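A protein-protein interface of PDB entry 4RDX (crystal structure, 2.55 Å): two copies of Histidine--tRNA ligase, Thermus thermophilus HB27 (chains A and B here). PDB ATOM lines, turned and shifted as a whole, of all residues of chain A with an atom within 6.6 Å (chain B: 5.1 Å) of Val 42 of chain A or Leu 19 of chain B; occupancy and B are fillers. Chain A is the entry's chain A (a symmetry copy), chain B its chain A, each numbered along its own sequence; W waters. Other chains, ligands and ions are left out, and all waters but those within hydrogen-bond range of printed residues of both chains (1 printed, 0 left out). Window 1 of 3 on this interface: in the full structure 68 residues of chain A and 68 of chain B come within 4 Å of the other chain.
OE1 of Glu 40 of chain A sits at hydrogen-bond distance from NE2 of Gln 23 of chain B.
The backbone carbonyl oxygen of Val 42 of chain A lies within hydrogen-bond range of the backbone NH of Leu 14 of chain B (2.9 Å).
NH1 of Arg 30 of chain A lies close to NE2 of Gln 23 of chain B (3.3 Å).
The side-chain carboxylate of Asp 13 of chain B is in salt-bridge range of the guanidinium group of Arg 90 of chain A (2.7 Å).
The backbone carbonyl oxygen (O) of Trp 107 of chain A sits at hydrogen-bond distance from the backbone NH (N) of Leu 41 of chain A (2.9 Å).
OG1 of Thr 43 of chain A sits close to SD of Met 108 of chain A, 3.7 Å away.
The guanidinium group (NH1) of Arg 81 of chain A sits at hydrogen-bond distance from the backbone carbonyl oxygen (O) of Pro 44 of chain A.
NH1 of Arg 81 of chain A sits at hydrogen-bond distance from O of Thr 43 of chain A (3.1 Å).
OE2 of Glu 40 of chain A lies within salt-bridge range of NH1 of Arg 30 of chain A (3.3 Å).
Among the printed residues, merely in contact across the chains: Glu 40 of chain A with Phe 15 of chain B (3.1 Å), Thr 43 of chain A with Asp 13 of chain B (3.3 Å), Val 42 of chain A with Asp 13 of chain B (3.3 Å), Leu 41 of chain A with Phe 15 of chain B (3.5 Å), Glu 40 of chain A with Leu 19 of chain B (3.6 Å), Pro 44 of chain A with Asp 13 of chain B (3.6 Å), Leu 41 of chain A with Leu 14 of chain B (3.6 Å), Val 42 of chain A with Leu 19 of chain B (3.8 Å), Leu 41 of chain A with Asp 13 of chain B (3.98 Å) and Pro 44 of chain A with Lys 12 of chain B (3.99 Å).
Of chain B, only Asp 13, Leu 14 and Leu 19 come within 4 Å of Val 42 of chain A.
Of chain A, only Glu 40 (3.6 Å) and Val 42 (3.8 Å) come within 4 Å of Leu 19 of chain B.
Of the printed residues of chain B, Arg 90 of chain A touches Asp 13 (2.7 Å).
Of the printed residues of chain A, Phe 15 of chain B touches Glu 40 and Leu 41.
Printed residues of chain A within 4 Å of Lys 12 of chain B: Pro 44.
Printed residues of chain B within 4 Å of Thr 43 of chain A: Asp 13 (3.3 Å).
Printed residues of chain A within 4 Å of Gln 23 of chain B: Arg 30 and Glu 40.
Arg 24 of chain B touches none of the printed residues of chain A.
Met 21 of chain B touches none of the printed residues of chain A.
The nearest residue of chain B that does not touch Val 42 of chain A is Lys 12 of chain B (4.2 Å).
The nearest residue of chain A that does not touch Leu 19 of chain B is Leu 41 of chain A (4.8 Å).
Printed residues of chain A that touch a printed residue of chain B: Arg 30, Glu 40, Leu 41, Val 42, Thr 43, Pro 44 and Arg 90.
Hydrophobic or aromatic side chains of chain A that line the printed part of chain B: Leu 41, Val 42 and Pro 44.
Of the 13 printed residues of chain B, 6 touch a printed residue of chain A.
Among the printed residues, 14 pairs touch across the chains.
No position is printed for both chains.
Of the 14 pairs that touch across the chains among the printed residues, none has its exchanged pair printed and touching as well.
Water W1 bridges O of Glu 40 of chain A and N of Gly 16 of chain B.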
ATOM      1  N   ARG A  30     -22.765 -22.974  -5.220  1.00  0.00           N
ATOM      2  CA  ARG A  30     -21.582 -23.795  -5.457  1.00  0.00           C
ATOM      3  C   ARG A  30     -21.037 -24.321  -4.145  1.00  0.00           C
ATOM      4  O   ARG A  30     -20.811 -25.520  -3.998  1.00  0.00           O
ATOM      5  CB  ARG A  30     -20.488 -22.988  -6.152  1.00  0.00           C
ATOM      6  CG  ARG A  30     -19.194 -23.764  -6.353  1.00  0.00           C
ATOM      7  CD  ARG A  30     -18.132 -22.891  -6.983  1.00  0.00           C
ATOM      8  NE  ARG A  30     -18.706 -22.090  -8.057  1.00  0.00           N
ATOM      9  CZ  ARG A  30     -18.826 -22.508  -9.310  1.00  0.00           C
ATOM     10  NH1 ARG A  30     -18.397 -23.716  -9.643  1.00  0.00           N
ATOM     11  NH2 ARG A  30     -19.369 -21.719 -10.224  1.00  0.00           N
ATOM     12  N   GLU A  40     -19.736 -30.307 -10.329  1.00  0.00           N
ATOM     13  CA  GLU A  40     -20.256 -29.343 -11.304  1.00  0.00           C
ATOM     14  C   GLU A  40     -20.207 -29.852 -12.742  1.00  0.00           C
ATOM     15  O   GLU A  40     -19.228 -30.464 -13.173  1.00  0.00           O
ATOM     16  CB  GLU A  40     -19.572 -27.975 -11.197  1.00  0.00           C
ATOM     17  CG  GLU A  40     -20.233 -26.901 -12.068  1.00  0.00           C
ATOM     18  CD  GLU A  40     -19.719 -25.508 -11.769  1.00  0.00           C
ATOM     19  OE1 GLU A  40     -18.661 -25.397 -11.116  1.00  0.00           O
ATOM     20  OE2 GLU A  40     -20.378 -24.525 -12.170  1.00  0.00           O
ATOM     21  N   LEU A  41     -21.290 -29.586 -13.466  1.00  0.00           N
ATOM     22  CA  LEU A  41     -21.448 -30.008 -14.843  1.00  0.00           C
ATOM     23  C   LEU A  41     -21.877 -28.786 -15.647  1.00  0.00           C
ATOM     24  O   LEU A  41     -22.583 -27.922 -15.130  1.00  0.00           O
ATOM     25  CB  LEU A  41     -22.533 -31.084 -14.910  1.00  0.00           C
ATOM     26  CG  LEU A  41     -22.323 -32.349 -15.744  1.00  0.00           C
ATOM     27  CD1 LEU A  41     -22.346 -32.038 -17.229  1.00  0.00           C
ATOM     28  CD2 LEU A  41     -21.025 -33.029 -15.356  1.00  0.00           C
ATOM     29  N   VAL A  42     -21.427 -28.696 -16.894  1.00  0.00           N
ATOM     30  CA  VAL A  42     -21.970 -27.715 -17.828  1.00  0.00           C
ATOM     31  C   VAL A  42     -22.310 -28.410 -19.137  1.00  0.00           C
ATOM     32  O   VAL A  42     -21.434 -28.947 -19.811  1.00  0.00           O
ATOM     33  CB  VAL A  42     -21.006 -26.536 -18.099  1.00  0.00           C
ATOM     34  CG1 VAL A  42     -21.587 -25.614 -19.168  1.00  0.00           C
ATOM     35  CG2 VAL A  42     -20.735 -25.756 -16.819  1.00  0.00           C
ATOM     36  N   THR A  43     -23.593 -28.401 -19.482  1.00  0.00           N
ATOM     37  CA  THR A  43     -24.079 -29.036 -20.699  1.00  0.00           C
ATOM     38  C   THR A  43     -24.272 -27.958 -21.764  1.00  0.00           C
ATOM     39  O   THR A  43     -24.311 -26.774 -21.435  1.00  0.00           O
ATOM     40  CB  THR A  43     -25.404 -29.778 -20.426  1.00  0.00           C
ATOM     41  OG1 THR A  43     -26.483 -28.838 -20.362  1.00  0.00           O
ATOM     42  CG2 THR A  43     -25.320 -30.547 -19.120  1.00  0.00           C
ATOM     43  N   PRO A  44     -24.376 -28.354 -23.047  1.00  0.00           N
ATOM     44  CA  PRO A  44     -24.504 -27.352 -24.114  1.00  0.00           C
ATOM     45  C   PRO A  44     -25.807 -26.558 -24.042  1.00  0.00           C
ATOM     46  O   PRO A  44     -26.744 -26.972 -23.361  1.00  0.00           O
ATOM     47  CB  PRO A  44     -24.474 -28.197 -25.391  1.00  0.00           C
ATOM     48  CG  PRO A  44     -23.796 -29.468 -24.996  1.00  0.00           C
ATOM     49  CD  PRO A  44     -24.253 -29.716 -23.593  1.00  0.00           C
ATOM     50  N   ILE A  45     -25.856 -25.431 -24.745  1.00  0.00           N
ATOM     51  CA  ILE A  45     -27.021 -24.556 -24.717  1.00  0.00           C
ATOM     52  C   ILE A  45     -28.195 -25.149 -25.500  1.00  0.00           C
ATOM     53  O   ILE A  45     -29.355 -24.977 -25.121  1.00  0.00           O
ATOM     54  CB  ILE A  45     -26.666 -23.122 -25.198  1.00  0.00           C
ATOM     55  CG1 ILE A  45     -26.618 -22.161 -24.008  1.00  0.00           C
ATOM     56  CG2 ILE A  45     -27.659 -22.617 -26.234  1.00  0.00           C
ATOM     57  CD1 ILE A  45     -25.620 -22.555 -22.943  1.00  0.00           C
ATOM     58  N   ARG A  81     -32.182 -25.259 -24.651  1.00  0.00           N
ATOM     59  CA  ARG A  81     -32.428 -25.834 -23.331  1.00  0.00           C
ATOM     60  C   ARG A  81     -33.540 -25.117 -22.560  1.00  0.00           C
ATOM     61  O   ARG A  81     -33.403 -23.943 -22.218  1.00  0.00           O
ATOM     62  CB  ARG A  81     -31.120 -25.776 -22.531  1.00  0.00           C
ATOM     63  CG  ARG A  81     -30.977 -26.783 -21.405  1.00  0.00           C
ATOM     64  CD  ARG A  81     -29.591 -26.679 -20.778  1.00  0.00           C
ATOM     65  NE  ARG A  81     -29.260 -25.304 -20.409  1.00  0.00           N
ATOM     66  CZ  ARG A  81     -28.020 -24.861 -20.220  1.00  0.00           C
ATOM     67  NH1 ARG A  81     -26.987 -25.682 -20.370  1.00  0.00           N
ATOM     68  NH2 ARG A  81     -27.808 -23.596 -19.885  1.00  0.00           N
ATOM     69  N   ARG A  90     -28.916 -37.003 -19.482  1.00  0.00           N
ATOM     70  CA  ARG A  90     -28.246 -37.315 -20.740  1.00  0.00           C
ATOM     71  C   ARG A  90     -26.730 -37.332 -20.531  1.00  0.00           C
ATOM     72  O   ARG A  90     -26.028 -38.169 -21.095  1.00  0.00           O
ATOM     73  CB  ARG A  90     -28.639 -36.310 -21.829  1.00  0.00           C
ATOM     74  CG  ARG A  90     -28.345 -36.766 -23.259  1.00  0.00           C
ATOM     75  CD  ARG A  90     -26.932 -36.407 -23.688  1.00  0.00           C
ATOM     76  NE  ARG A  90     -26.664 -34.985 -23.508  1.00  0.00           N
ATOM     77  CZ  ARG A  90     -25.527 -34.492 -23.028  1.00  0.00           C
ATOM     78  NH1 ARG A  90     -24.542 -35.309 -22.678  1.00  0.00           N
ATOM     79  NH2 ARG A  90     -25.373 -33.182 -22.895  1.00  0.00           N
ATOM     80  N   TRP A 107     -24.360 -30.815 -10.094  1.00  0.00           N
ATOM     81  CA  TRP A 107     -25.028 -29.520 -10.078  1.00  0.00           C
ATOM     82  C   TRP A 107     -24.588 -28.666 -11.257  1.00  0.00           C
ATOM     83  O   TRP A 107     -23.509 -28.864 -11.812  1.00  0.00           O
ATOM     84  CB  TRP A 107     -24.841 -28.790  -8.739  1.00  0.00           C
ATOM     85  CG  TRP A 107     -23.539 -28.077  -8.572  1.00  0.00           C
ATOM     86  CD1 TRP A 107     -22.373 -28.599  -8.090  1.00  0.00           C
ATOM     87  CD2 TRP A 107     -23.273 -26.701  -8.861  1.00  0.00           C
ATOM     88  NE1 TRP A 107     -21.394 -27.634  -8.070  1.00  0.00           N
ATOM     89  CE2 TRP A 107     -21.921 -26.460  -8.541  1.00  0.00           C
ATOM     90  CE3 TRP A 107     -24.045 -25.648  -9.365  1.00  0.00           C
ATOM     91  CZ2 TRP A 107     -21.327 -25.212  -8.706  1.00  0.00           C
ATOM     92  CZ3 TRP A 107     -23.453 -24.411  -9.528  1.00  0.00           C
ATOM     93  CH2 TRP A 107     -22.106 -24.203  -9.199  1.00  0.00           C
ATOM     94  N   MET A 108     -25.442 -27.728 -11.646  1.00  0.00           N
ATOM     95  CA  MET A 108     -25.192 -26.919 -12.830  1.00  0.00           C
ATOM     96  C   MET A 108     -25.834 -25.552 -12.672  1.00  0.00           C
ATOM     97  O   MET A 108     -26.911 -25.435 -12.111  1.00  0.00           O
ATOM     98  CB  MET A 108     -25.772 -27.612 -14.065  1.00  0.00           C
ATOM     99  CG  MET A 108     -25.535 -26.886 -15.371  1.00  0.00           C
ATOM    100  SD  MET A 108     -26.141 -27.831 -16.781  1.00  0.00           S
ATOM    101  CE  MET A 108     -27.910 -27.758 -16.492  1.00  0.00           C
ATOM    102  N   ALA A 109     -25.176 -24.511 -13.159  1.00  0.00           N
ATOM    103  CA  ALA A 109     -25.781 -23.188 -13.129  1.00  0.00           C
ATOM    104  C   ALA A 109     -25.676 -22.539 -14.497  1.00  0.00           C
ATOM    105  O   ALA A 109     -24.582 -22.437 -15.055  1.00  0.00           O
ATOM    106  CB  ALA A 109     -25.129 -22.323 -12.069  1.00  0.00           C
ATOM    107  N   LYS B  12     -19.717 -30.181 -26.344  1.00  0.00           N
ATOM    108  CA  LYS B  12     -19.307 -31.133 -25.319  1.00  0.00           C
ATOM    109  C   LYS B  12     -19.774 -30.702 -23.933  1.00  0.00           C
ATOM    110  O   LYS B  12     -20.027 -29.523 -23.689  1.00  0.00           O
ATOM    111  CB  LYS B  12     -17.783 -31.289 -25.317  1.00  0.00           C
ATOM    112  N   ASP B  13     -19.892 -31.667 -23.028  1.00  0.00           N
ATOM    113  CA  ASP B  13     -20.130 -31.356 -21.629  1.00  0.00           C
ATOM    114  C   ASP B  13     -18.798 -30.953 -21.004  1.00  0.00           C
ATOM    115  O   ASP B  13     -17.731 -31.240 -21.554  1.00  0.00           O
ATOM    116  CB  ASP B  13     -20.747 -32.551 -20.900  1.00  0.00           C
ATOM    117  CG  ASP B  13     -22.135 -32.892 -21.416  1.00  0.00           C
ATOM    118  OD1 ASP B  13     -23.079 -32.119 -21.140  1.00  0.00           O
ATOM    119  OD2 ASP B  13     -22.287 -33.929 -22.096  1.00  0.00           O
ATOM    120  N   LEU B  14     -18.857 -30.283 -19.858  1.00  0.00           N
ATOM    121  CA  LEU B  14     -17.654 -29.745 -19.235  1.00  0.00           C
ATOM    122  C   LEU B  14     -17.670 -30.007 -17.736  1.00  0.00           C
ATOM    123  O   LEU B  14     -18.579 -29.560 -17.036  1.00  0.00           O
ATOM    124  CB  LEU B  14     -17.569 -28.245 -19.493  1.00  0.00           C
ATOM    125  CG  LEU B  14     -16.238 -27.596 -19.832  1.00  0.00           C
ATOM    126  CD1 LEU B  14     -15.583 -28.311 -21.011  1.00  0.00           C
ATOM    127  CD2 LEU B  14     -16.477 -26.124 -20.138  1.00  0.00           C
ATOM    128  N   PHE B  15     -16.664 -30.729 -17.248  1.00  0.00           N
ATOM    129  CA  PHE B  15     -16.524 -30.980 -15.814  1.00  0.00           C
ATOM    130  C   PHE B  15     -15.118 -31.451 -15.459  1.00  0.00           C
ATOM    131  O   PHE B  15     -14.326 -31.799 -16.336  1.00  0.00           O
ATOM    132  CB  PHE B  15     -17.564 -31.998 -15.325  1.00  0.00           C
ATOM    133  CG  PHE B  15     -17.465 -33.348 -15.983  1.00  0.00           C
ATOM    134  CD1 PHE B  15     -18.093 -33.594 -17.193  1.00  0.00           C
ATOM    135  CD2 PHE B  15     -16.769 -34.382 -15.378  1.00  0.00           C
ATOM    136  CE1 PHE B  15     -18.017 -34.835 -17.794  1.00  0.00           C
ATOM    137  CE2 PHE B  15     -16.690 -35.627 -15.975  1.00  0.00           C
ATOM    138  CZ  PHE B  15     -17.316 -35.854 -17.185  1.00  0.00           C
ATOM    139  N   GLY B  16     -14.819 -31.465 -14.163  1.00  0.00           N
ATOM    140  CA  GLY B  16     -13.525 -31.907 -13.686  1.00  0.00           C
ATOM    141  C   GLY B  16     -12.435 -30.884 -13.931  1.00  0.00           C
ATOM    142  O   GLY B  16     -12.646 -29.686 -13.744  1.00  0.00           O
ATOM    143  N   LYS B  17     -11.270 -31.354 -14.365  1.00  0.00           N
ATOM    144  CA  LYS B  17     -10.128 -30.476 -14.609  1.00  0.00           C
ATOM    145  C   LYS B  17     -10.344 -29.462 -15.735  1.00  0.00           C
ATOM    146  O   LYS B  17      -9.868 -28.338 -15.647  1.00  0.00           O
ATOM    147  CB  LYS B  17      -8.863 -31.297 -14.872  1.00  0.00           C
ATOM    148  CG  LYS B  17      -8.231 -31.866 -13.614  1.00  0.00           C
ATOM    149  CD  LYS B  17      -6.886 -32.507 -13.904  1.00  0.00           C
ATOM    150  CE  LYS B  17      -6.260 -33.064 -12.635  1.00  0.00           C
ATOM    151  NZ  LYS B  17      -4.877 -33.583 -12.841  1.00  0.00           N
ATOM    152  N   GLU B  18     -11.053 -29.852 -16.790  1.00  0.00           N
ATOM    153  CA  GLU B  18     -11.272 -28.954 -17.928  1.00  0.00           C
ATOM    154  C   GLU B  18     -12.140 -27.745 -17.545  1.00  0.00           C
ATOM    155  O   GLU B  18     -11.831 -26.603 -17.898  1.00  0.00           O
ATOM    156  CB  GLU B  18     -11.883 -29.718 -19.109  1.00  0.00           C
ATOM    157  CG  GLU B  18     -11.898 -28.941 -20.421  1.00  0.00           C
ATOM    158  CD  GLU B  18     -12.208 -29.820 -21.621  1.00  0.00           C
ATOM    159  OE1 GLU B  18     -12.312 -31.052 -21.450  1.00  0.00           O
ATOM    160  OE2 GLU B  18     -12.343 -29.275 -22.736  1.00  0.00           O
ATOM    161  N   LEU B  19     -13.229 -28.003 -16.829  1.00  0.00           N
ATOM    162  CA  LEU B  19     -14.100 -26.940 -16.332  1.00  0.00           C
ATOM    163  C   LEU B  19     -13.353 -25.995 -15.394  1.00  0.00           C
ATOM    164  O   LEU B  19     -13.457 -24.771 -15.516  1.00  0.00           O
ATOM    165  CB  LEU B  19     -15.291 -27.544 -15.599  1.00  0.00           C
ATOM    166  CG  LEU B  19     -16.241 -26.525 -14.976  1.00  0.00           C
ATOM    167  CD1 LEU B  19     -16.988 -25.777 -16.066  1.00  0.00           C
ATOM    168  CD2 LEU B  19     -17.202 -27.191 -14.012  1.00  0.00           C
ATOM    169  N   ARG B  20     -12.608 -26.572 -14.454  1.00  0.00           N
ATOM    170  CA  ARG B  20     -11.770 -25.796 -13.544  1.00  0.00           C
ATOM    171  C   ARG B  20     -10.790 -24.941 -14.337  1.00  0.00           C
ATOM    172  O   ARG B  20     -10.464 -23.814 -13.951  1.00  0.00           O
ATOM    173  CB  ARG B  20     -10.999 -26.717 -12.595  1.00  0.00           C
ATOM    174  CG  ARG B  20     -11.783 -27.194 -11.378  1.00  0.00           C
ATOM    175  CD  ARG B  20     -10.856 -27.388 -10.179  1.00  0.00           C
ATOM    176  NE  ARG B  20      -9.941 -28.514 -10.351  1.00  0.00           N
ATOM    177  CZ  ARG B  20      -8.738 -28.592  -9.790  1.00  0.00           C
ATOM    178  NH1 ARG B  20      -8.294 -27.601  -9.028  1.00  0.00           N
ATOM    179  NH2 ARG B  20      -7.976 -29.655  -9.998  1.00  0.00           N
ATOM    180  N   MET B  21     -10.333 -25.504 -15.452  1.00  0.00           N
ATOM    181  CA  MET B  21      -9.428 -24.836 -16.368  1.00  0.00           C
ATOM    182  C   MET B  21     -10.064 -23.566 -16.910  1.00  0.00           C
ATOM    183  O   MET B  21      -9.519 -22.457 -16.755  1.00  0.00           O
ATOM    184  CB  MET B  21      -9.053 -25.780 -17.511  1.00  0.00           C
ATOM    185  CG  MET B  21      -7.767 -25.424 -18.233  1.00  0.00           C
ATOM    186  SD  MET B  21      -6.247 -25.483 -17.249  1.00  0.00           S
ATOM    187  CE  MET B  21      -6.151 -23.859 -16.523  1.00  0.00           C
ATOM    188  N   HIS B  22     -11.232 -23.742 -17.526  1.00  0.00           N
ATOM    189  CA  HIS B  22     -12.027 -22.633 -18.048  1.00  0.00           C
ATOM    190  C   HIS B  22     -12.254 -21.542 -17.002  1.00  0.00           C
ATOM    191  O   HIS B  22     -12.055 -20.347 -17.270  1.00  0.00           O
ATOM    192  CB  HIS B  22     -13.368 -23.154 -18.575  1.00  0.00           C
ATOM    193  CG  HIS B  22     -13.269 -23.829 -19.906  1.00  0.00           C
ATOM    194  ND1 HIS B  22     -14.251 -23.725 -20.868  1.00  0.00           N
ATOM    195  CD2 HIS B  22     -12.298 -24.606 -20.444  1.00  0.00           C
ATOM    196  CE1 HIS B  22     -13.892 -24.414 -21.938  1.00  0.00           C
ATOM    197  NE2 HIS B  22     -12.709 -24.957 -21.704  1.00  0.00           N
ATOM    198  N   GLN B  23     -12.663 -21.972 -15.811  1.00  0.00           N
ATOM    199  CA  GLN B  23     -12.931 -21.074 -14.695  1.00  0.00           C
ATOM    200  C   GLN B  23     -11.713 -20.248 -14.263  1.00  0.00           C
ATOM    201  O   GLN B  23     -11.828 -19.042 -14.026  1.00  0.00           O
ATOM    202  CB  GLN B  23     -13.475 -21.873 -13.514  1.00  0.00           C
ATOM    203  CG  GLN B  23     -14.905 -22.351 -13.708  1.00  0.00           C
ATOM    204  CD  GLN B  23     -15.362 -23.257 -12.590  1.00  0.00           C
ATOM    205  OE1 GLN B  23     -14.546 -23.888 -11.918  1.00  0.00           O
ATOM    206  NE2 GLN B  23     -16.672 -23.327 -12.383  1.00  0.00           N
ATOM    207  N   ARG B  24     -10.556 -20.899 -14.149  1.00  0.00           N
ATOM    208  CA  ARG B  24      -9.307 -20.205 -13.824  1.00  0.00           C
ATOM    209  C   ARG B  24      -8.982 -19.149 -14.879  1.00  0.00           C
ATOM    210  O   ARG B  24      -8.619 -18.008 -14.548  1.00  0.00           O
ATOM    211  CB  ARG B  24      -8.140 -21.196 -13.690  1.00  0.00           C
ATOM    212  CG  ARG B  24      -6.831 -20.548 -13.237  1.00  0.00           C
ATOM    213  CD  ARG B  24      -5.737 -21.571 -12.865  1.00  0.00           C
ATOM    214  NE  ARG B  24      -5.100 -22.159 -14.036  1.00  0.00           N
ATOM    215  CZ  ARG B  24      -3.999 -21.684 -14.608  1.00  0.00           C
ATOM    216  NH1 ARG B  24      -3.395 -20.609 -14.109  1.00  0.00           N
ATOM    217  NH2 ARG B  24      -3.505 -22.288 -15.683  1.00  0.00           N
HETATM  218  O   HOH W   1     -16.640 -30.348 -12.341  1.00  0.00           O
